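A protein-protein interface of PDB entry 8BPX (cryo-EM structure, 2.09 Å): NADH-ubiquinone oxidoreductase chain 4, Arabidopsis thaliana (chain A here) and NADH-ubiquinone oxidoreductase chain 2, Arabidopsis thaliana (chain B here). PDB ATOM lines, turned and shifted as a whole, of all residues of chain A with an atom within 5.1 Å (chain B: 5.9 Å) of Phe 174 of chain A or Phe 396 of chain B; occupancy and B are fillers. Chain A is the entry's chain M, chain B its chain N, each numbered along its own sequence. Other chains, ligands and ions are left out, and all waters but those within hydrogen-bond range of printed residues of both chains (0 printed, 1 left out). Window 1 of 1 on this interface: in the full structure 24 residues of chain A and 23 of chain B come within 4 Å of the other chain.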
ATOM      1  N   LEU A 150      13.565 -24.071  11.061  1.00  0.00           N
ATOM      2  CA  LEU A 150      12.417 -24.968  11.126  1.00  0.00           C
ATOM      3  C   LEU A 150      11.162 -24.313  10.569  1.00  0.00           C
ATOM      4  O   LEU A 150      10.367 -24.971   9.899  1.00  0.00           O
ATOM      5  CB  LEU A 150      12.173 -25.417  12.564  1.00  0.00           C
ATOM      6  CG  LEU A 150      12.750 -26.770  12.963  1.00  0.00           C
ATOM      7  CD1 LEU A 150      14.171 -26.901  12.442  1.00  0.00           C
ATOM      8  CD2 LEU A 150      12.701 -26.928  14.470  1.00  0.00           C
ATOM      9  N   ILE A 151      10.967 -23.027  10.836  1.00  0.00           N
ATOM     10  CA  ILE A 151       9.754 -22.325  10.415  1.00  0.00           C
ATOM     11  C   ILE A 151       9.667 -22.257   8.889  1.00  0.00           C
ATOM     12  O   ILE A 151       8.680 -22.757   8.317  1.00  0.00           O
ATOM     13  CB  ILE A 151       9.677 -20.931  11.065  1.00  0.00           C
ATOM     14  CG1 ILE A 151       9.546 -21.069  12.586  1.00  0.00           C
ATOM     15  CG2 ILE A 151       8.530 -20.121  10.482  1.00  0.00           C
ATOM     16  CD1 ILE A 151       9.593 -19.757  13.337  1.00  0.00           C
ATOM     17  N   PHE A 154       9.305 -25.845   7.446  1.00  0.00           N
ATOM     18  CA  PHE A 154       7.940 -26.301   7.671  1.00  0.00           C
ATOM     19  C   PHE A 154       7.005 -25.742   6.612  1.00  0.00           C
ATOM     20  O   PHE A 154       6.227 -26.482   5.997  1.00  0.00           O
ATOM     21  CB  PHE A 154       7.502 -25.872   9.078  1.00  0.00           C
ATOM     22  CG  PHE A 154       6.178 -26.434   9.523  1.00  0.00           C
ATOM     23  CD1 PHE A 154       5.996 -27.797   9.671  1.00  0.00           C
ATOM     24  CD2 PHE A 154       5.124 -25.588   9.827  1.00  0.00           C
ATOM     25  CE1 PHE A 154       4.782 -28.309  10.093  1.00  0.00           C
ATOM     26  CE2 PHE A 154       3.908 -26.093  10.247  1.00  0.00           C
ATOM     27  CZ  PHE A 154       3.737 -27.457  10.380  1.00  0.00           C
ATOM     28  N   ILE A 155       7.093 -24.430   6.373  1.00  0.00           N
ATOM     29  CA  ILE A 155       6.236 -23.798   5.373  1.00  0.00           C
ATOM     30  C   ILE A 155       6.514 -24.367   3.986  1.00  0.00           C
ATOM     31  O   ILE A 155       5.589 -24.660   3.221  1.00  0.00           O
ATOM     32  CB  ILE A 155       6.411 -22.268   5.404  1.00  0.00           C
ATOM     33  CG1 ILE A 155       6.063 -21.721   6.791  1.00  0.00           C
ATOM     34  CG2 ILE A 155       5.550 -21.606   4.332  1.00  0.00           C
ATOM     35  CD1 ILE A 155       4.665 -22.063   7.246  1.00  0.00           C
ATOM     36  N   ALA A 169       4.443 -35.479   7.003  1.00  0.00           N
ATOM     37  CA  ALA A 169       5.881 -35.302   6.825  1.00  0.00           C
ATOM     38  C   ALA A 169       6.372 -34.042   7.530  1.00  0.00           C
ATOM     39  O   ALA A 169       7.392 -34.063   8.232  1.00  0.00           O
ATOM     40  CB  ALA A 169       6.217 -35.255   5.335  1.00  0.00           C
ATOM     41  N   ALA A 170       5.647 -32.935   7.364  1.00  0.00           N
ATOM     42  CA  ALA A 170       6.039 -31.674   7.979  1.00  0.00           C
ATOM     43  C   ALA A 170       5.935 -31.736   9.498  1.00  0.00           C
ATOM     44  O   ALA A 170       6.840 -31.267  10.204  1.00  0.00           O
ATOM     45  CB  ALA A 170       5.183 -30.538   7.421  1.00  0.00           C
ATOM     46  N   TYR A 171       4.839 -32.302  10.020  1.00  0.00           N
ATOM     47  CA  TYR A 171       4.721 -32.480  11.465  1.00  0.00           C
ATOM     48  C   TYR A 171       5.922 -33.240  12.021  1.00  0.00           C
ATOM     49  O   TYR A 171       6.541 -32.820  13.007  1.00  0.00           O
ATOM     50  CB  TYR A 171       3.433 -33.227  11.818  1.00  0.00           C
ATOM     51  CG  TYR A 171       2.167 -32.399  11.840  1.00  0.00           C
ATOM     52  CD1 TYR A 171       2.173 -31.077  12.266  1.00  0.00           C
ATOM     53  CD2 TYR A 171       0.954 -32.959  11.463  1.00  0.00           C
ATOM     54  CE1 TYR A 171       1.004 -30.333  12.295  1.00  0.00           C
ATOM     55  CE2 TYR A 171      -0.210 -32.228  11.488  1.00  0.00           C
ATOM     56  CZ  TYR A 171      -0.186 -30.917  11.905  1.00  0.00           C
ATOM     57  OH  TYR A 171      -1.356 -30.196  11.927  1.00  0.00           O
ATOM     58  N   GLN A 172       6.259 -34.372  11.397  1.00  0.00           N
ATOM     59  CA  GLN A 172       7.344 -35.201  11.911  1.00  0.00           C
ATOM     60  C   GLN A 172       8.686 -34.486  11.829  1.00  0.00           C
ATOM     61  O   GLN A 172       9.480 -34.544  12.776  1.00  0.00           O
ATOM     62  CB  GLN A 172       7.397 -36.525  11.156  1.00  0.00           C
ATOM     63  CG  GLN A 172       6.722 -37.663  11.883  1.00  0.00           C
ATOM     64  CD  GLN A 172       6.434 -38.832  10.977  1.00  0.00           C
ATOM     65  OE1 GLN A 172       5.279 -39.158  10.712  1.00  0.00           O
ATOM     66  NE2 GLN A 172       7.488 -39.468  10.485  1.00  0.00           N
ATOM     67  N   PHE A 173       8.957 -33.812  10.708  1.00  0.00           N
ATOM     68  CA  PHE A 173      10.189 -33.041  10.586  1.00  0.00           C
ATOM     69  C   PHE A 173      10.312 -32.046  11.730  1.00  0.00           C
ATOM     70  O   PHE A 173      11.307 -32.043  12.472  1.00  0.00           O
ATOM     71  CB  PHE A 173      10.215 -32.318   9.236  1.00  0.00           C
ATOM     72  CG  PHE A 173      11.258 -31.238   9.138  1.00  0.00           C
ATOM     73  CD1 PHE A 173      12.593 -31.558   8.959  1.00  0.00           C
ATOM     74  CD2 PHE A 173      10.904 -29.902   9.241  1.00  0.00           C
ATOM     75  CE1 PHE A 173      13.554 -30.566   8.870  1.00  0.00           C
ATOM     76  CE2 PHE A 173      11.861 -28.905   9.155  1.00  0.00           C
ATOM     77  CZ  PHE A 173      13.189 -29.241   8.969  1.00  0.00           C
ATOM     78  N   PHE A 174       9.270 -31.230  11.921  1.00  0.00           N
ATOM     79  CA  PHE A 174       9.321 -30.185  12.938  1.00  0.00           C
ATOM     80  C   PHE A 174       9.522 -30.781  14.325  1.00  0.00           C
ATOM     81  O   PHE A 174      10.372 -30.319  15.092  1.00  0.00           O
ATOM     82  CB  PHE A 174       8.048 -29.340  12.891  1.00  0.00           C
ATOM     83  CG  PHE A 174       8.234 -27.924  13.369  1.00  0.00           C
ATOM     84  CD1 PHE A 174       8.669 -27.657  14.657  1.00  0.00           C
ATOM     85  CD2 PHE A 174       7.971 -26.858  12.529  1.00  0.00           C
ATOM     86  CE1 PHE A 174       8.841 -26.358  15.093  1.00  0.00           C
ATOM     87  CE2 PHE A 174       8.141 -25.557  12.959  1.00  0.00           C
ATOM     88  CZ  PHE A 174       8.574 -25.307  14.244  1.00  0.00           C
ATOM     89  N   LEU A 175       8.771 -31.836  14.654  1.00  0.00           N
ATOM     90  CA  LEU A 175       8.785 -32.339  16.025  1.00  0.00           C
ATOM     91  C   LEU A 175      10.092 -33.060  16.353  1.00  0.00           C
ATOM     92  O   LEU A 175      10.669 -32.842  17.427  1.00  0.00           O
ATOM     93  CB  LEU A 175       7.578 -33.247  16.254  1.00  0.00           C
ATOM     94  CG  LEU A 175       6.251 -32.480  16.307  1.00  0.00           C
ATOM     95  CD1 LEU A 175       5.057 -33.408  16.152  1.00  0.00           C
ATOM     96  CD2 LEU A 175       6.142 -31.679  17.590  1.00  0.00           C
ATOM     97  N   TYR A 176      10.580 -33.915  15.446  1.00  0.00           N
ATOM     98  CA  TYR A 176      11.871 -34.564  15.662  1.00  0.00           C
ATOM     99  C   TYR A 176      12.978 -33.531  15.838  1.00  0.00           C
ATOM    100  O   TYR A 176      13.761 -33.588  16.804  1.00  0.00           O
ATOM    101  CB  TYR A 176      12.198 -35.484  14.487  1.00  0.00           C
ATOM    102  CG  TYR A 176      11.799 -36.927  14.670  1.00  0.00           C
ATOM    103  CD1 TYR A 176      12.664 -37.835  15.268  1.00  0.00           C
ATOM    104  CD2 TYR A 176      10.570 -37.388  14.228  1.00  0.00           C
ATOM    105  CE1 TYR A 176      12.311 -39.156  15.429  1.00  0.00           C
ATOM    106  CE2 TYR A 176      10.206 -38.708  14.383  1.00  0.00           C
ATOM    107  CZ  TYR A 176      11.080 -39.589  14.983  1.00  0.00           C
ATOM    108  OH  TYR A 176      10.720 -40.904  15.141  1.00  0.00           O
ATOM    109  N   THR A 177      13.051 -32.568  14.912  1.00  0.00           N
ATOM    110  CA  THR A 177      14.130 -31.594  14.969  1.00  0.00           C
ATOM    111  C   THR A 177      14.040 -30.742  16.228  1.00  0.00           C
ATOM    112  O   THR A 177      15.064 -30.436  16.850  1.00  0.00           O
ATOM    113  CB  THR A 177      14.113 -30.722  13.716  1.00  0.00           C
ATOM    114  OG1 THR A 177      13.989 -31.554  12.557  1.00  0.00           O
ATOM    115  CG2 THR A 177      15.400 -29.954  13.621  1.00  0.00           C
ATOM    116  N   LEU A 178      12.823 -30.369  16.637  1.00  0.00           N
ATOM    117  CA  LEU A 178      12.672 -29.555  17.838  1.00  0.00           C
ATOM    118  C   LEU A 178      13.058 -30.330  19.092  1.00  0.00           C
ATOM    119  O   LEU A 178      13.651 -29.761  20.016  1.00  0.00           O
ATOM    120  CB  LEU A 178      11.240 -29.033  17.945  1.00  0.00           C
ATOM    121  CG  LEU A 178      10.886 -28.390  19.287  1.00  0.00           C
ATOM    122  CD1 LEU A 178      11.448 -26.982  19.373  1.00  0.00           C
ATOM    123  CD2 LEU A 178       9.391 -28.387  19.512  1.00  0.00           C
ATOM    124  N   LEU A 179      12.718 -31.620  19.158  1.00  0.00           N
ATOM    125  CA  LEU A 179      13.139 -32.432  20.298  1.00  0.00           C
ATOM    126  C   LEU A 179      14.659 -32.456  20.420  1.00  0.00           C
ATOM    127  O   LEU A 179      15.221 -32.211  21.502  1.00  0.00           O
ATOM    128  CB  LEU A 179      12.583 -33.851  20.159  1.00  0.00           C
ATOM    129  CG  LEU A 179      12.579 -34.749  21.401  1.00  0.00           C
ATOM    130  CD1 LEU A 179      11.839 -34.097  22.560  1.00  0.00           C
ATOM    131  CD2 LEU A 179      11.978 -36.103  21.079  1.00  0.00           C
ATOM    132  N   PHE B 391      -0.604 -14.295  12.127  1.00  0.00           N
ATOM    133  CA  PHE B 391      -1.160 -15.256  13.095  1.00  0.00           C
ATOM    134  C   PHE B 391      -0.119 -16.391  13.299  1.00  0.00           C
ATOM    135  O   PHE B 391       0.009 -16.869  14.356  1.00  0.00           O
ATOM    136  CB  PHE B 391      -2.562 -15.678  12.627  1.00  0.00           C
ATOM    137  CG  PHE B 391      -3.393 -16.347  13.687  1.00  0.00           C
ATOM    138  CD1 PHE B 391      -3.090 -16.179  15.024  1.00  0.00           C
ATOM    139  CD2 PHE B 391      -4.524 -17.070  13.356  1.00  0.00           C
ATOM    140  CE1 PHE B 391      -3.873 -16.749  16.008  1.00  0.00           C
ATOM    141  CE2 PHE B 391      -5.298 -17.657  14.340  1.00  0.00           C
ATOM    142  CZ  PHE B 391      -4.967 -17.501  15.662  1.00  0.00           C
ATOM    143  N   SER B 392       0.565 -16.786  12.238  1.00  0.00           N
ATOM    144  CA  SER B 392       1.631 -17.812  12.266  1.00  0.00           C
ATOM    145  C   SER B 392       2.807 -17.365  13.163  1.00  0.00           C
ATOM    146  O   SER B 392       3.273 -18.165  13.919  1.00  0.00           O
ATOM    147  CB  SER B 392       2.068 -18.125  10.846  1.00  0.00           C
ATOM    148  OG  SER B 392       1.006 -18.717  10.135  1.00  0.00           O
ATOM    149  N   ILE B 393       3.183 -16.104  13.069  1.00  0.00           N
ATOM    150  CA  ILE B 393       4.258 -15.536  13.939  1.00  0.00           C
ATOM    151  C   ILE B 393       3.802 -15.645  15.406  1.00  0.00           C
ATOM    152  O   ILE B 393       4.535 -16.218  16.174  1.00  0.00           O
ATOM    153  CB  ILE B 393       4.607 -14.116  13.488  1.00  0.00           C
ATOM    154  CG1 ILE B 393       5.366 -14.086  12.161  1.00  0.00           C
ATOM    155  CG2 ILE B 393       5.350 -13.360  14.579  1.00  0.00           C
ATOM    156  CD1 ILE B 393       5.348 -12.714  11.535  1.00  0.00           C
ATOM    157  N   THR B 394       2.576 -15.195  15.715  1.00  0.00           N
ATOM    158  CA  THR B 394       2.006 -15.371  17.074  1.00  0.00           C
ATOM    159  C   THR B 394       2.125 -16.855  17.530  1.00  0.00           C
ATOM    160  O   THR B 394       2.640 -17.065  18.557  1.00  0.00           O
ATOM    161  CB  THR B 394       0.587 -14.751  17.192  1.00  0.00           C
ATOM    162  OG1 THR B 394       0.496 -13.588  16.368  1.00  0.00           O
ATOM    163  CG2 THR B 394       0.158 -14.486  18.616  1.00  0.00           C
ATOM    164  N   MET B 395       1.658 -17.820  16.744  1.00  0.00           N
ATOM    165  CA  MET B 395       1.726 -19.279  17.070  1.00  0.00           C
ATOM    166  C   MET B 395       3.173 -19.742  17.297  1.00  0.00           C
ATOM    167  O   MET B 395       3.419 -20.474  18.226  1.00  0.00           O
ATOM    168  CB  MET B 395       1.128 -20.122  15.954  1.00  0.00           C
ATOM    169  CG  MET B 395      -0.333 -19.929  15.736  1.00  0.00           C
ATOM    170  SD  MET B 395      -1.256 -20.510  17.143  1.00  0.00           S
ATOM    171  CE  MET B 395      -1.641 -18.967  17.972  1.00  0.00           C
ATOM    172  N   PHE B 396       4.055 -19.340  16.401  1.00  0.00           N
ATOM    173  CA  PHE B 396       5.430 -19.774  16.622  1.00  0.00           C
ATOM    174  C   PHE B 396       6.012 -19.132  17.872  1.00  0.00           C
ATOM    175  O   PHE B 396       6.807 -19.763  18.577  1.00  0.00           O
ATOM    176  CB  PHE B 396       6.293 -19.461  15.399  1.00  0.00           C
ATOM    177  CG  PHE B 396       6.038 -20.364  14.225  1.00  0.00           C
ATOM    178  CD1 PHE B 396       6.162 -21.737  14.344  1.00  0.00           C
ATOM    179  CD2 PHE B 396       5.678 -19.835  12.995  1.00  0.00           C
ATOM    180  CE1 PHE B 396       5.927 -22.564  13.262  1.00  0.00           C
ATOM    181  CE2 PHE B 396       5.437 -20.657  11.913  1.00  0.00           C
ATOM    182  CZ  PHE B 396       5.564 -22.021  12.046  1.00  0.00           C
ATOM    183  N   SER B 397       5.628 -17.886  18.164  1.00  0.00           N
ATOM    184  CA  SER B 397       6.040 -17.257  19.414  1.00  0.00           C
ATOM    185  C   SER B 397       5.453 -17.981  20.620  1.00  0.00           C
ATOM    186  O   SER B 397       6.149 -18.200  21.619  1.00  0.00           O
ATOM    187  CB  SER B 397       5.628 -15.786  19.418  1.00  0.00           C
ATOM    188  OG  SER B 397       6.351 -15.060  20.392  1.00  0.00           O
ATOM    189  N   TYR B 398       4.173 -18.359  20.544  1.00  0.00           N
ATOM    190  CA  TYR B 398       3.571 -19.162  21.606  1.00  0.00           C
ATOM    191  C   TYR B 398       4.332 -20.466  21.801  1.00  0.00           C
ATOM    192  O   TYR B 398       4.534 -20.916  22.933  1.00  0.00           O
ATOM    193  CB  TYR B 398       2.104 -19.460  21.287  1.00  0.00           C
ATOM    194  CG  TYR B 398       1.110 -18.463  21.831  1.00  0.00           C
ATOM    195  CD1 TYR B 398       0.998 -18.229  23.194  1.00  0.00           C
ATOM    196  CD2 TYR B 398       0.263 -17.770  20.978  1.00  0.00           C
ATOM    197  CE1 TYR B 398       0.081 -17.321  23.689  1.00  0.00           C
ATOM    198  CE2 TYR B 398      -0.658 -16.863  21.464  1.00  0.00           C
ATOM    199  CZ  TYR B 398      -0.744 -16.642  22.818  1.00  0.00           C
ATOM    200  OH  TYR B 398      -1.660 -15.741  23.300  1.00  0.00           O
ATOM    201  N   ALA B 399       4.754 -21.090  20.701  1.00  0.00           N
ATOM    202  CA  ALA B 399       5.526 -22.321  20.783  1.00  0.00           C
ATOM    203  C   ALA B 399       6.918 -22.090  21.353  1.00  0.00           C
ATOM    204  O   ALA B 399       7.562 -23.048  21.788  1.00  0.00           O
ATOM    205  CB  ALA B 399       5.625 -22.971  19.403  1.00  0.00           C
ATOM    206  N   GLY B 400       7.385 -20.845  21.371  1.00  0.00           N
ATOM    207  CA  GLY B 400       8.696 -20.531  21.896  1.00  0.00           C
ATOM    208  C   GLY B 400       9.836 -20.703  20.921  1.00  0.00           C
ATOM    209  O   GLY B 400      10.987 -20.818  21.350  1.00  0.00           O
ATOM    210  N   ILE B 401       9.560 -20.720  19.622  1.00  0.00           N
ATOM    211  CA  ILE B 401      10.607 -20.905  18.619  1.00  0.00           C
ATOM    212  C   ILE B 401      11.464 -19.647  18.558  1.00  0.00           C
ATOM    213  O   ILE B 401      10.935 -18.544  18.361  1.00  0.00           O
ATOM    214  CB  ILE B 401      10.019 -21.236  17.238  1.00  0.00           C
ATOM    215  CG1 ILE B 401       9.067 -22.428  17.328  1.00  0.00           C
ATOM    216  CG2 ILE B 401      11.136 -21.512  16.242  1.00  0.00           C
ATOM    217  CD1 ILE B 401       9.696 -23.674  17.912  1.00  0.00           C
ATOM    218  N   LEU B 404      11.949 -15.580  18.154  1.00  0.00           N
ATOM    219  CA  LEU B 404      10.752 -14.854  18.555  1.00  0.00           C
ATOM    220  C   LEU B 404      10.736 -14.632  20.065  1.00  0.00           C
ATOM    221  O   LEU B 404      11.395 -15.338  20.832  1.00  0.00           O
ATOM    222  CB  LEU B 404       9.497 -15.602  18.111  1.00  0.00           C
ATOM    223  CG  LEU B 404       9.401 -15.827  16.600  1.00  0.00           C
ATOM    224  CD1 LEU B 404       8.179 -16.643  16.260  1.00  0.00           C
ATOM    225  CD2 LEU B 404       9.395 -14.509  15.844  1.00  0.00           C
ATOM    226  N   CYS B 437       4.219 -27.149  20.837  1.00  0.00           N
ATOM    227  CA  CYS B 437       4.603 -26.844  19.467  1.00  0.00           C
ATOM    228  C   CYS B 437       3.705 -27.568  18.477  1.00  0.00           C
ATOM    229  O   CYS B 437       3.310 -26.993  17.457  1.00  0.00           O
ATOM    230  CB  CYS B 437       6.065 -27.207  19.226  1.00  0.00           C
ATOM    231  SG  CYS B 437       6.606 -26.899  17.536  1.00  0.00           S
ATOM    232  N   TYR B 440       0.308 -25.823  18.369  1.00  0.00           N
ATOM    233  CA  TYR B 440       0.409 -24.480  17.806  1.00  0.00           C
ATOM    234  C   TYR B 440       0.620 -24.522  16.297  1.00  0.00           C
ATOM    235  O   TYR B 440       0.013 -23.736  15.564  1.00  0.00           O
ATOM    236  CB  TYR B 440       1.543 -23.697  18.469  1.00  0.00           C
ATOM    237  CG  TYR B 440       1.245 -23.246  19.877  1.00  0.00           C
ATOM    238  CD1 TYR B 440       0.082 -22.547  20.173  1.00  0.00           C
ATOM    239  CD2 TYR B 440       2.127 -23.519  20.912  1.00  0.00           C
ATOM    240  CE1 TYR B 440      -0.192 -22.138  21.461  1.00  0.00           C
ATOM    241  CE2 TYR B 440       1.857 -23.124  22.202  1.00  0.00           C
ATOM    242  CZ  TYR B 440       0.699 -22.432  22.471  1.00  0.00           C
ATOM    243  OH  TYR B 440       0.437 -22.031  23.756  1.00  0.00           O
ATOM    244  N   ILE B 441       1.471 -25.431  15.810  1.00  0.00           N
ATOM    245  CA  ILE B 441       1.695 -25.515  14.368  1.00  0.00           C
ATOM    246  C   ILE B 441       0.550 -26.198  13.641  1.00  0.00           C
ATOM    247  O   ILE B 441       0.478 -26.112  12.409  1.00  0.00           O
ATOM    248  CB  ILE B 441       3.018 -26.232  14.034  1.00  0.00           C
ATOM    249  CG1 ILE B 441       2.945 -27.713  14.403  1.00  0.00           C
ATOM    250  CG2 ILE B 441       4.195 -25.538  14.714  1.00  0.00           C
ATOM    251  CD1 ILE B 441       4.089 -28.525  13.848  1.00  0.00           C
ATOM    252  N   VAL B 444      -1.112 -23.336  11.983  1.00  0.00           N
ATOM    253  CA  VAL B 444      -0.381 -22.922  10.792  1.00  0.00           C
ATOM    254  C   VAL B 444      -0.662 -23.879   9.641  1.00  0.00           C
ATOM    255  O   VAL B 444      -0.873 -23.454   8.499  1.00  0.00           O
ATOM    256  CB  VAL B 444       1.126 -22.814  11.094  1.00  0.00           C
ATOM    257  CG1 VAL B 444       1.883 -22.358   9.859  1.00  0.00           C
ATOM    258  CG2 VAL B 444       1.363 -21.857  12.259  1.00  0.00           C
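Hydrophobic or aromatic side chains of chain B within 4 Å of the printed part of chain A: Phe 396, Ile 401, Ile 441 and Val 444. Hydrophobic or aromatic side chains of chain A within 4 Å of the printed part of chain B: Ile 151, Phe 154, Ile 155, Tyr 171, Phe 174 and Leu 178. Among the printed residues, 9 pairs touch across the chains.
Printed residues of chain B within 4 Å of Ile 155 of chain A: Val 444 (3.8 Å). Ala 169 of chain A touches none of the printed residues of chain B. Printed residues of chain B within 4 Å of Tyr 171 of chain A: Ile 441. Of the printed residues of chain B, Phe 174 of chain A touches Phe 396 (3.7 Å), Ile 401 (3.99 Å) and Cys 437 (3.4 Å). Phe 396 of chain B touches just these residues of chain A: Ile 151 and Phe 174. Ser 397 of chain B touches none of the printed residues of chain A. Of the printed residues of chain A, Ile 401 of chain B touches Ile 151 and Phe 174. The nearest printed residue of chain B that does not touch Phe 154 of chain A is Phe 396 of chain B (4.2 Å).
Ile 151 of chain A touches Phe 396 of chain B. Ile 151 of chain A touches Ile 401 of chain B. CD1 of Ile 441 of chain B touches CZ of Phe 154 of chain A, at 3.6 Å. Val 444 of chain B touches Ile 155 of chain A. CD1 of Ile 441 of chain B touches CD1 of Tyr 171 of chain A, at 3.6 Å. Phe 174 of chain A touches Phe 396 of chain B (CE2 to CE1, 3.7 Å). Phe 174 of chain A touches Ile 401 of chain B (CE1 to CD1, 3.99 Å). Phe 174 of chain A touches Cys 437 of chain B (CE1 to SG, 3.4 Å). Leu 178 of chain A touches Cys 437 of chain B (CD2 to CB, 3.5 Å).
The backbone carbonyl oxygen (O) of Phe 396 of chain B lies within hydrogen-bond range of the backbone NH (N) of Ile 401 of chain B (3.1 Å).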
